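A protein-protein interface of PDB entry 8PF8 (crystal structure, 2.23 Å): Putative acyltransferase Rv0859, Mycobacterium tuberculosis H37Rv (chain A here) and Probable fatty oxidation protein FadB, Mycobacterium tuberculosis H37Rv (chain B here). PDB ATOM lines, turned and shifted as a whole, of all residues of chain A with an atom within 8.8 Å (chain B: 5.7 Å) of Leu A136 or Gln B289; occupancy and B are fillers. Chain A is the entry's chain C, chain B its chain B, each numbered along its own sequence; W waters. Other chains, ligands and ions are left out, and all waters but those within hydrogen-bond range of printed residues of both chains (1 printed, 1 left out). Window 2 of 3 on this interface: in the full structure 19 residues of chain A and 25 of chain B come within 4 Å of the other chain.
Of the 12 printed residues of chain B, 4 touch a printed residue of chain A. Hydrophobic or aromatic side chains of chain B within 4 Å of the printed part of chain A: Pro B249, Leu B258 and Val B285. Of the 14 printed residues of chain A, 3 touch a printed residue of chain B. Hydrophobic or aromatic side chains of chain A within 4 Å of the printed part of chain B: Leu A136 and Pro A138. Among the printed residues, 5 pairs touch across the chains.
Of the printed residues of chain B, Leu A136 touches Pro B249 (3.5 Å), Val B285 (3.99 Å) and Gln B289 (3.6 Å). Of chain A, only Leu A136 (3.6 Å) comes within 4 Å of Gln B289. No residue of chain A comes within 4 Å of Gly B287. No residue of chain A comes within 4 Å of Ala B288. No residue of chain A comes within 4 Å of Val B290. Of the printed residues of chain A, Leu B258 touches Gly A135. Printed residues of chain B within 4 Å of Gly A135: Leu B258 (3.7 Å). Of the printed residues of chain A, Pro B249 touches Leu A136. The nearest printed residue of chain B that does not touch Leu A136 is Leu B258 (4.3 Å). The nearest residue of chain A that does not touch Gln B289 is Asp A137 (5.9 Å).
Water W1 lies within hydrogen-bond range of the side-chain carboxylate of Asp A137 (2.6 Å) and the side-chain carboxylate of Glu B286 (3.3 Å).
Leu B258 touches Gly A135. Leu A136 touches Pro B249. Val B285 touches Leu A136 (CG1 to O, 3.99 Å). Leu A136 touches Gln B289 (CD2 to NE2, 3.6 Å). CG2 of Val B285 touches CG of Pro A138 (3.6 Å).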
ATOM      1  N   GLY A 128      11.561   6.028 -11.289  1.00  0.00           N
ATOM      2  CA  GLY A 128      12.286   6.993 -10.491  1.00  0.00           C
ATOM      3  C   GLY A 128      13.783   6.786 -10.435  1.00  0.00           C
ATOM      4  O   GLY A 128      14.472   7.564  -9.763  1.00  0.00           O
ATOM      5  N   SER A 129      14.311   5.768 -11.123  1.00  0.00           N
ATOM      6  CA  SER A 129      15.748   5.515 -11.110  1.00  0.00           C
ATOM      7  C   SER A 129      16.536   6.652 -11.745  1.00  0.00           C
ATOM      8  O   SER A 129      17.713   6.844 -11.415  1.00  0.00           O
ATOM      9  CB  SER A 129      16.058   4.207 -11.837  1.00  0.00           C
ATOM     10  OG  SER A 129      15.320   3.133 -11.287  1.00  0.00           O
ATOM     11  N   ASP A 130      15.922   7.404 -12.659  1.00  0.00           N
ATOM     12  CA  ASP A 130      16.602   8.480 -13.370  1.00  0.00           C
ATOM     13  C   ASP A 130      16.683   9.770 -12.568  1.00  0.00           C
ATOM     14  O   ASP A 130      17.045  10.806 -13.132  1.00  0.00           O
ATOM     15  CB  ASP A 130      15.910   8.755 -14.712  1.00  0.00           C
ATOM     16  CG  ASP A 130      14.432   9.063 -14.560  1.00  0.00           C
ATOM     17  OD1 ASP A 130      13.787   8.485 -13.659  1.00  0.00           O
ATOM     18  OD2 ASP A 130      13.910   9.879 -15.352  1.00  0.00           O
ATOM     19  N   GLY A 131      16.370   9.730 -11.278  1.00  0.00           N
ATOM     20  CA  GLY A 131      16.318  10.937 -10.482  1.00  0.00           C
ATOM     21  C   GLY A 131      15.079  11.749 -10.792  1.00  0.00           C
ATOM     22  O   GLY A 131      13.954  11.270 -10.620  1.00  0.00           O
ATOM     23  N   GLY A 132      15.270  12.974 -11.268  1.00  0.00           N
ATOM     24  CA  GLY A 132      14.146  13.832 -11.569  1.00  0.00           C
ATOM     25  C   GLY A 132      14.408  15.280 -11.216  1.00  0.00           C
ATOM     26  O   GLY A 132      14.833  15.593 -10.100  1.00  0.00           O
ATOM     27  N   ALA A 133      14.145  16.175 -12.168  1.00  0.00           N
ATOM     28  CA  ALA A 133      14.382  17.598 -11.964  1.00  0.00           C
ATOM     29  C   ALA A 133      13.501  18.203 -10.876  1.00  0.00           C
ATOM     30  O   ALA A 133      13.755  19.341 -10.469  1.00  0.00           O
ATOM     31  CB  ALA A 133      14.182  18.344 -13.286  1.00  0.00           C
ATOM     32  N   MET A 134      12.488  17.481 -10.390  1.00  0.00           N
ATOM     33  CA  MET A 134      11.610  17.984  -9.333  1.00  0.00           C
ATOM     34  C   MET A 134      12.057  17.506  -7.952  1.00  0.00           C
ATOM     35  O   MET A 134      12.348  18.324  -7.073  1.00  0.00           O
ATOM     36  CB  MET A 134      10.159  17.567  -9.606  1.00  0.00           C
ATOM     37  CG  MET A 134       9.438  18.456 -10.604  1.00  0.00           C
ATOM     38  SD  MET A 134       9.312  20.153 -10.009  1.00  0.00           S
ATOM     39  CE  MET A 134       8.722  20.979 -11.481  1.00  0.00           C
ATOM     40  N   GLY A 135      12.116  16.186  -7.752  1.00  0.00           N
ATOM     41  CA  GLY A 135      12.542  15.616  -6.482  1.00  0.00           C
ATOM     42  C   GLY A 135      13.892  16.103  -5.984  1.00  0.00           C
ATOM     43  O   GLY A 135      14.124  16.103  -4.770  1.00  0.00           O
ATOM     44  N   LEU A 136      14.789  16.509  -6.888  1.00  0.00           N
ATOM     45  CA  LEU A 136      16.085  17.087  -6.537  1.00  0.00           C
ATOM     46  C   LEU A 136      16.054  18.604  -6.442  1.00  0.00           C
ATOM     47  O   LEU A 136      17.108  19.223  -6.258  1.00  0.00           O
ATOM     48  CB  LEU A 136      17.145  16.675  -7.564  1.00  0.00           C
ATOM     49  CG  LEU A 136      17.603  15.224  -7.469  1.00  0.00           C
ATOM     50  CD1 LEU A 136      18.049  14.690  -8.811  1.00  0.00           C
ATOM     51  CD2 LEU A 136      18.726  15.132  -6.473  1.00  0.00           C
ATOM     52  N   ASP A 137      14.880  19.215  -6.570  1.00  0.00           N
ATOM     53  CA  ASP A 137      14.727  20.668  -6.563  1.00  0.00           C
ATOM     54  C   ASP A 137      13.557  21.008  -5.651  1.00  0.00           C
ATOM     55  O   ASP A 137      12.428  21.218  -6.116  1.00  0.00           O
ATOM     56  CB  ASP A 137      14.512  21.199  -7.981  1.00  0.00           C
ATOM     57  CG  ASP A 137      14.589  22.707  -8.061  1.00  0.00           C
ATOM     58  OD1 ASP A 137      14.839  23.355  -7.022  1.00  0.00           O
ATOM     59  OD2 ASP A 137      14.399  23.246  -9.173  1.00  0.00           O
ATOM     60  N   PRO A 138      13.791  21.064  -4.336  1.00  0.00           N
ATOM     61  CA  PRO A 138      12.692  21.380  -3.408  1.00  0.00           C
ATOM     62  C   PRO A 138      12.006  22.703  -3.694  1.00  0.00           C
ATOM     63  O   PRO A 138      10.806  22.829  -3.426  1.00  0.00           O
ATOM     64  CB  PRO A 138      13.390  21.393  -2.040  1.00  0.00           C
ATOM     65  CG  PRO A 138      14.564  20.501  -2.215  1.00  0.00           C
ATOM     66  CD  PRO A 138      15.033  20.720  -3.623  1.00  0.00           C
ATOM     67  N   ALA A 139      12.726  23.692  -4.231  1.00  0.00           N
ATOM     68  CA  ALA A 139      12.110  24.986  -4.512  1.00  0.00           C
ATOM     69  C   ALA A 139      10.967  24.854  -5.511  1.00  0.00           C
ATOM     70  O   ALA A 139       9.911  25.475  -5.342  1.00  0.00           O
ATOM     71  CB  ALA A 139      13.160  25.968  -5.030  1.00  0.00           C
ATOM     72  N   THR A 140      11.156  24.051  -6.558  1.00  0.00           N
ATOM     73  CA  THR A 140      10.111  23.876  -7.558  1.00  0.00           C
ATOM     74  C   THR A 140       9.139  22.762  -7.196  1.00  0.00           C
ATOM     75  O   THR A 140       7.952  22.860  -7.529  1.00  0.00           O
ATOM     76  CB  THR A 140      10.727  23.605  -8.934  1.00  0.00           C
ATOM     77  OG1 THR A 140      11.568  22.446  -8.869  1.00  0.00           O
ATOM     78  CG2 THR A 140      11.548  24.806  -9.398  1.00  0.00           C
ATOM     79  N   ASN A 141       9.613  21.707  -6.530  1.00  0.00           N
ATOM     80  CA  ASN A 141       8.704  20.706  -5.977  1.00  0.00           C
ATOM     81  C   ASN A 141       7.694  21.361  -5.042  1.00  0.00           C
ATOM     82  O   ASN A 141       6.490  21.086  -5.116  1.00  0.00           O
ATOM     83  CB  ASN A 141       9.509  19.624  -5.249  1.00  0.00           C
ATOM     84  CG  ASN A 141       8.649  18.467  -4.747  1.00  0.00           C
ATOM     85  OD1 ASN A 141       7.579  18.663  -4.172  1.00  0.00           O
ATOM     86  ND2 ASN A 141       9.135  17.248  -4.951  1.00  0.00           N
ATOM     87  N   ARG B 174      26.602  19.632   6.359  1.00  0.00           N
ATOM     88  CA  ARG B 174      27.829  18.848   6.239  1.00  0.00           C
ATOM     89  C   ARG B 174      28.109  18.039   7.500  1.00  0.00           C
ATOM     90  O   ARG B 174      28.785  17.006   7.432  1.00  0.00           O
ATOM     91  CB  ARG B 174      29.017  19.761   5.927  1.00  0.00           C
ATOM     92  CG  ARG B 174      29.032  20.332   4.515  1.00  0.00           C
ATOM     93  CD  ARG B 174      28.979  19.232   3.472  1.00  0.00           C
ATOM     94  NE  ARG B 174      29.627  19.617   2.223  1.00  0.00           N
ATOM     95  CZ  ARG B 174      29.003  20.140   1.175  1.00  0.00           C
ATOM     96  NH1 ARG B 174      27.705  20.393   1.199  1.00  0.00           N
ATOM     97  NH2 ARG B 174      29.699  20.413   0.076  1.00  0.00           N
ATOM     98  N   PRO B 249      22.172  13.855  -2.297  1.00  0.00           N
ATOM     99  CA  PRO B 249      20.938  13.689  -3.084  1.00  0.00           C
ATOM    100  C   PRO B 249      21.052  12.657  -4.196  1.00  0.00           C
ATOM    101  O   PRO B 249      20.032  12.087  -4.604  1.00  0.00           O
ATOM    102  CB  PRO B 249      20.694  15.097  -3.638  1.00  0.00           C
ATOM    103  CG  PRO B 249      21.295  15.994  -2.625  1.00  0.00           C
ATOM    104  CD  PRO B 249      22.522  15.278  -2.128  1.00  0.00           C
ATOM    105  N   SER B 250      22.261  12.398  -4.700  1.00  0.00           N
ATOM    106  CA  SER B 250      22.468  11.341  -5.682  1.00  0.00           C
ATOM    107  C   SER B 250      22.518   9.953  -5.053  1.00  0.00           C
ATOM    108  O   SER B 250      22.413   8.959  -5.780  1.00  0.00           O
ATOM    109  CB  SER B 250      23.757  11.591  -6.471  1.00  0.00           C
ATOM    110  OG  SER B 250      24.893  11.568  -5.623  1.00  0.00           O
ATOM    111  N   LEU B 258      13.697  11.748  -0.790  1.00  0.00           N
ATOM    112  CA  LEU B 258      13.894  13.187  -0.959  1.00  0.00           C
ATOM    113  C   LEU B 258      12.710  13.913  -1.592  1.00  0.00           C
ATOM    114  O   LEU B 258      12.469  15.073  -1.212  1.00  0.00           O
ATOM    115  CB  LEU B 258      15.173  13.432  -1.774  1.00  0.00           C
ATOM    116  CG  LEU B 258      15.770  14.838  -1.736  1.00  0.00           C
ATOM    117  CD1 LEU B 258      16.016  15.271  -0.304  1.00  0.00           C
ATOM    118  CD2 LEU B 258      17.067  14.868  -2.522  1.00  0.00           C
ATOM    119  N   ALA B 284      19.638  23.810   1.504  1.00  0.00           N
ATOM    120  CA  ALA B 284      20.256  22.621   2.081  1.00  0.00           C
ATOM    121  C   ALA B 284      20.453  21.536   1.029  1.00  0.00           C
ATOM    122  O   ALA B 284      21.542  20.961   0.913  1.00  0.00           O
ATOM    123  CB  ALA B 284      19.404  22.103   3.241  1.00  0.00           C
ATOM    124  N   VAL B 285      19.410  21.247   0.249  1.00  0.00           N
ATOM    125  CA  VAL B 285      19.497  20.191  -0.755  1.00  0.00           C
ATOM    126  C   VAL B 285      20.422  20.607  -1.894  1.00  0.00           C
ATOM    127  O   VAL B 285      21.304  19.844  -2.306  1.00  0.00           O
ATOM    128  CB  VAL B 285      18.092  19.822  -1.266  1.00  0.00           C
ATOM    129  CG1 VAL B 285      18.179  18.853  -2.437  1.00  0.00           C
ATOM    130  CG2 VAL B 285      17.266  19.217  -0.140  1.00  0.00           C
ATOM    131  N   GLU B 286      20.239  21.825  -2.417  1.00  0.00           N
ATOM    132  CA  GLU B 286      21.100  22.296  -3.500  1.00  0.00           C
ATOM    133  C   GLU B 286      22.555  22.354  -3.059  1.00  0.00           C
ATOM    134  O   GLU B 286      23.465  22.077  -3.849  1.00  0.00           O
ATOM    135  CB  GLU B 286      20.645  23.671  -3.988  1.00  0.00           C
ATOM    136  CG  GLU B 286      19.273  23.698  -4.624  1.00  0.00           C
ATOM    137  CD  GLU B 286      18.925  25.069  -5.166  1.00  0.00           C
ATOM    138  OE1 GLU B 286      19.851  25.786  -5.607  1.00  0.00           O
ATOM    139  OE2 GLU B 286      17.731  25.433  -5.145  1.00  0.00           O
ATOM    140  N   GLY B 287      22.793  22.717  -1.797  1.00  0.00           N
ATOM    141  CA  GLY B 287      24.150  22.775  -1.288  1.00  0.00           C
ATOM    142  C   GLY B 287      24.813  21.416  -1.174  1.00  0.00           C
ATOM    143  O   GLY B 287      26.020  21.293  -1.403  1.00  0.00           O
ATOM    144  N   ALA B 288      24.043  20.381  -0.823  1.00  0.00           N
ATOM    145  CA  ALA B 288      24.582  19.029  -0.728  1.00  0.00           C
ATOM    146  C   ALA B 288      24.971  18.446  -2.079  1.00  0.00           C
ATOM    147  O   ALA B 288      25.671  17.428  -2.111  1.00  0.00           O
ATOM    148  CB  ALA B 288      23.569  18.101  -0.054  1.00  0.00           C
ATOM    149  N   GLN B 289      24.534  19.052  -3.185  1.00  0.00           N
ATOM    150  CA  GLN B 289      24.835  18.550  -4.520  1.00  0.00           C
ATOM    151  C   GLN B 289      26.169  19.037  -5.063  1.00  0.00           C
ATOM    152  O   GLN B 289      26.616  18.530  -6.097  1.00  0.00           O
ATOM    153  CB  GLN B 289      23.731  18.956  -5.503  1.00  0.00           C
ATOM    154  CG  GLN B 289      22.353  18.415  -5.175  1.00  0.00           C
ATOM    155  CD  GLN B 289      21.325  18.769  -6.233  1.00  0.00           C
ATOM    156  OE1 GLN B 289      20.784  19.875  -6.247  1.00  0.00           O
ATOM    157  NE2 GLN B 289      21.051  17.829  -7.129  1.00  0.00           N
ATOM    158  N   VAL B 290      26.809  20.007  -4.410  1.00  0.00           N
ATOM    159  CA  VAL B 290      28.015  20.642  -4.920  1.00  0.00           C
ATOM    160  C   VAL B 290      29.049  20.716  -3.800  1.00  0.00           C
ATOM    161  O   VAL B 290      28.824  20.252  -2.683  1.00  0.00           O
ATOM    162  CB  VAL B 290      27.736  22.045  -5.500  1.00  0.00           C
ATOM    163  CG1 VAL B 290      26.833  21.947  -6.722  1.00  0.00           C
ATOM    164  CG2 VAL B 290      27.113  22.944  -4.441  1.00  0.00           C
ATOM    165  N   ASP B 291      30.198  21.309  -4.121  1.00  0.00           N
ATOM    166  CA  ASP B 291      31.264  21.474  -3.147  1.00  0.00           C
ATOM    167  C   ASP B 291      30.858  22.487  -2.077  1.00  0.00           C
ATOM    168  O   ASP B 291      29.828  23.158  -2.173  1.00  0.00           O
ATOM    169  CB  ASP B 291      32.557  21.914  -3.833  1.00  0.00           C
ATOM    170  CG  ASP B 291      32.388  23.194  -4.629  1.00  0.00           C
ATOM    171  OD1 ASP B 291      31.758  23.147  -5.706  1.00  0.00           O
ATOM    172  OD2 ASP B 291      32.874  24.250  -4.169  1.00  0.00           O
HETATM  173  O   HOH W   1      15.910  25.616  -7.883  1.00  0.00           O
